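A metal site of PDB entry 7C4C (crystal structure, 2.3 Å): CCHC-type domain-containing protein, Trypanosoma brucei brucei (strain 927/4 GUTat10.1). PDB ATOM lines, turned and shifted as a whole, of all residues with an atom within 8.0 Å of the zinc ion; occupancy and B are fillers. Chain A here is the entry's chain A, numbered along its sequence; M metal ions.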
ATOM      1  N   THR A 303      -2.201   9.493   1.559  1.00  0.00           N
ATOM      2  CA  THR A 303      -3.189  10.467   1.129  1.00  0.00           C
ATOM      3  C   THR A 303      -2.471  11.600   0.419  1.00  0.00           C
ATOM      4  O   THR A 303      -1.333  11.944   0.742  1.00  0.00           O
ATOM      5  CB  THR A 303      -4.001  10.993   2.311  1.00  0.00           C
ATOM      6  OG1 THR A 303      -3.126  11.298   3.412  1.00  0.00           O
ATOM      7  CG2 THR A 303      -5.043   9.964   2.749  1.00  0.00           C
ATOM      8  N   CYS A 304      -3.138  12.169  -0.589  1.00  0.00           N
ATOM      9  CA  CYS A 304      -2.478  13.110  -1.475  1.00  0.00           C
ATOM     10  C   CYS A 304      -2.539  14.521  -0.938  1.00  0.00           C
ATOM     11  O   CYS A 304      -3.560  14.953  -0.381  1.00  0.00           O
ATOM     12  CB  CYS A 304      -3.098  13.071  -2.876  1.00  0.00           C
ATOM     13  SG  CYS A 304      -2.112  14.033  -4.053  1.00  0.00           S
ATOM     14  N   GLU A 305      -1.439  15.263  -1.079  1.00  0.00           N
ATOM     15  CA  GLU A 305      -1.417  16.646  -0.626  1.00  0.00           C
ATOM     16  C   GLU A 305      -2.357  17.591  -1.383  1.00  0.00           C
ATOM     17  O   GLU A 305      -3.017  18.431  -0.769  1.00  0.00           O
ATOM     18  CB  GLU A 305       0.020  17.190  -0.687  1.00  0.00           C
ATOM     19  N   LYS A 306      -2.425  17.450  -2.707  1.00  0.00           N
ATOM     20  CA  LYS A 306      -3.251  18.344  -3.528  1.00  0.00           C
ATOM     21  C   LYS A 306      -4.513  17.873  -4.275  1.00  0.00           C
ATOM     22  O   LYS A 306      -5.062  18.646  -5.053  1.00  0.00           O
ATOM     23  CB  LYS A 306      -2.344  19.090  -4.515  1.00  0.00           C
ATOM     24  N   CYS A 307      -4.992  16.643  -4.070  1.00  0.00           N
ATOM     25  CA  CYS A 307      -6.178  16.239  -4.816  1.00  0.00           C
ATOM     26  C   CYS A 307      -7.148  15.388  -3.997  1.00  0.00           C
ATOM     27  O   CYS A 307      -8.340  15.304  -4.334  1.00  0.00           O
ATOM     28  CB  CYS A 307      -5.776  15.485  -6.087  1.00  0.00           C
ATOM     29  SG  CYS A 307      -5.079  13.820  -5.813  1.00  0.00           S
ATOM     30  N   GLY A 308      -6.666  14.748  -2.941  1.00  0.00           N
ATOM     31  CA  GLY A 308      -7.512  13.900  -2.132  1.00  0.00           C
ATOM     32  C   GLY A 308      -7.765  12.517  -2.707  1.00  0.00           C
ATOM     33  O   GLY A 308      -8.912  12.047  -2.697  1.00  0.00           O
ATOM     34  N   GLN A 309      -6.734  11.867  -3.232  1.00  0.00           N
ATOM     35  CA  GLN A 309      -6.827  10.488  -3.723  1.00  0.00           C
ATOM     36  C   GLN A 309      -5.735   9.659  -3.063  1.00  0.00           C
ATOM     37  O   GLN A 309      -4.616  10.143  -2.860  1.00  0.00           O
ATOM     38  CB  GLN A 309      -6.711  10.421  -5.254  1.00  0.00           C
ATOM     39  N   LEU A 310      -6.057   8.415  -2.733  1.00  0.00           N
ATOM     40  CA  LEU A 310      -5.110   7.549  -2.047  1.00  0.00           C
ATOM     41  C   LEU A 310      -4.127   6.932  -3.040  1.00  0.00           C
ATOM     42  O   LEU A 310      -4.531   6.416  -4.088  1.00  0.00           O
ATOM     43  CB  LEU A 310      -5.849   6.438  -1.296  1.00  0.00           C
ATOM     44  CG  LEU A 310      -6.967   6.784  -0.319  1.00  0.00           C
ATOM     45  CD1 LEU A 310      -8.293   7.013  -1.031  1.00  0.00           C
ATOM     46  CD2 LEU A 310      -7.106   5.683   0.724  1.00  0.00           C
ATOM     47  N   GLY A 311      -2.834   6.996  -2.719  1.00  0.00           N
ATOM     48  CA  GLY A 311      -1.839   6.321  -3.520  1.00  0.00           C
ATOM     49  C   GLY A 311      -0.590   7.108  -3.868  1.00  0.00           C
ATOM     50  O   GLY A 311       0.464   6.520  -4.099  1.00  0.00           O
ATOM     51  N   HIS A 312      -0.700   8.438  -3.915  1.00  0.00           N
ATOM     52  CA  HIS A 312       0.397   9.279  -4.387  1.00  0.00           C
ATOM     53  C   HIS A 312       0.515  10.530  -3.532  1.00  0.00           C
ATOM     54  O   HIS A 312      -0.482  11.037  -2.998  1.00  0.00           O
ATOM     55  CB  HIS A 312       0.216   9.661  -5.875  1.00  0.00           C
ATOM     56  CG  HIS A 312      -1.169  10.122  -6.219  1.00  0.00           C
ATOM     57  ND1 HIS A 312      -2.211   9.245  -6.469  1.00  0.00           N
ATOM     58  CD2 HIS A 312      -1.683  11.364  -6.345  1.00  0.00           C
ATOM     59  CE1 HIS A 312      -3.309   9.928  -6.735  1.00  0.00           C
ATOM     60  NE2 HIS A 312      -3.013  11.219  -6.671  1.00  0.00           N
ATOM     61  N   THR A 313       1.739  11.031  -3.406  1.00  0.00           N
ATOM     62  CA  THR A 313       2.019  12.241  -2.654  1.00  0.00           C
ATOM     63  C   THR A 313       1.875  13.456  -3.568  1.00  0.00           C
ATOM     64  O   THR A 313       1.323  13.386  -4.667  1.00  0.00           O
ATOM     65  CB  THR A 313       3.402  12.179  -2.012  1.00  0.00           C
ATOM     66  OG1 THR A 313       4.336  11.565  -2.925  1.00  0.00           O
ATOM     67  CG2 THR A 313       3.366  11.376  -0.705  1.00  0.00           C
ATOM     68  N   GLY A 314       2.366  14.614  -3.115  1.00  0.00           N
ATOM     69  CA  GLY A 314       2.365  15.785  -3.966  1.00  0.00           C
ATOM     70  C   GLY A 314       3.365  15.672  -5.096  1.00  0.00           C
ATOM     71  O   GLY A 314       3.074  16.056  -6.238  1.00  0.00           O
ATOM     72  N   THR A 315       4.566  15.132  -4.811  1.00  0.00           N
ATOM     73  CA  THR A 315       5.663  15.000  -5.785  1.00  0.00           C
ATOM     74  C   THR A 315       5.364  14.002  -6.917  1.00  0.00           C
ATOM     75  O   THR A 315       6.284  13.707  -7.684  1.00  0.00           O
ATOM     76  CB  THR A 315       6.958  14.589  -5.066  1.00  0.00           C
ATOM     77  N   SER A 316       4.128  13.505  -7.050  1.00  0.00           N
ATOM     78  CA  SER A 316       3.806  12.512  -8.068  1.00  0.00           C
ATOM     79  C   SER A 316       2.303  12.494  -8.356  1.00  0.00           C
ATOM     80  O   SER A 316       1.654  11.459  -8.214  1.00  0.00           O
ATOM     81  CB  SER A 316       4.288  11.130  -7.623  1.00  0.00           C
ATOM     82  OG  SER A 316       3.958  10.884  -6.266  1.00  0.00           O
ATOM     83  N   CYS A 317       1.767  13.641  -8.769  1.00  0.00           N
ATOM     84  CA  CYS A 317       0.353  13.767  -9.108  1.00  0.00           C
ATOM     85  C   CYS A 317       0.116  13.748 -10.619  1.00  0.00           C
ATOM     86  O   CYS A 317      -1.005  14.007 -11.070  1.00  0.00           O
ATOM     87  CB  CYS A 317      -0.219  15.047  -8.490  1.00  0.00           C
ATOM     88  SG  CYS A 317      -2.019  15.080  -8.342  1.00  0.00           S
ATOM     89  N   PHE A 318       1.133  13.433 -11.410  1.00  0.00           N
ATOM     90  CA  PHE A 318       1.005  13.342 -12.858  1.00  0.00           C
ATOM     91  C   PHE A 318       0.415  11.999 -13.270  1.00  0.00           C
ATOM     92  O   PHE A 318       0.575  10.991 -12.578  1.00  0.00           O
ATOM     93  CB  PHE A 318       2.363  13.544 -13.524  1.00  0.00           C
ATOM     94  CG  PHE A 318       3.433  12.617 -13.024  1.00  0.00           C
ATOM     95  CD1 PHE A 318       4.217  12.969 -11.940  1.00  0.00           C
ATOM     96  CD2 PHE A 318       3.637  11.390 -13.637  1.00  0.00           C
ATOM     97  CE1 PHE A 318       5.200  12.107 -11.468  1.00  0.00           C
ATOM     98  CE2 PHE A 318       4.608  10.533 -13.171  1.00  0.00           C
ATOM     99  CZ  PHE A 318       5.396  10.895 -12.089  1.00  0.00           C
HETATM  100 ZN    ZN M   1      -2.488  14.111  -6.315  1.00  0.00          ZN
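The zinc ion is bound by SG of Cys 304 (2.3 Å), SG of Cys 317 (2.3 Å) and SG of Cys 307 (2.7 Å).
The side-chain sulfur (SG) of Cys 304 sits close to the backbone carbonyl oxygen (O) of His 312, at 3.6 Å. SG of Cys 304 lies close to O of Thr 313 (3.5 Å). The side-chain sulfur (SG) of Cys 304 sits close to the backbone NH (N) of Lys 306. The backbone NH of Cys 304 lies close to the backbone carbonyl oxygen of Gln 309, 3.4 Å away. NE2 of His 312 sits close to SG of Cys 307, 3.4 Å away. SG of Cys 307 lies close to N of Gln 309 (3.6 Å).
Merely in contact with the zinc ion: His 312. Of the 16 residues printed, 4 come within 4 Å of the zinc ion.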
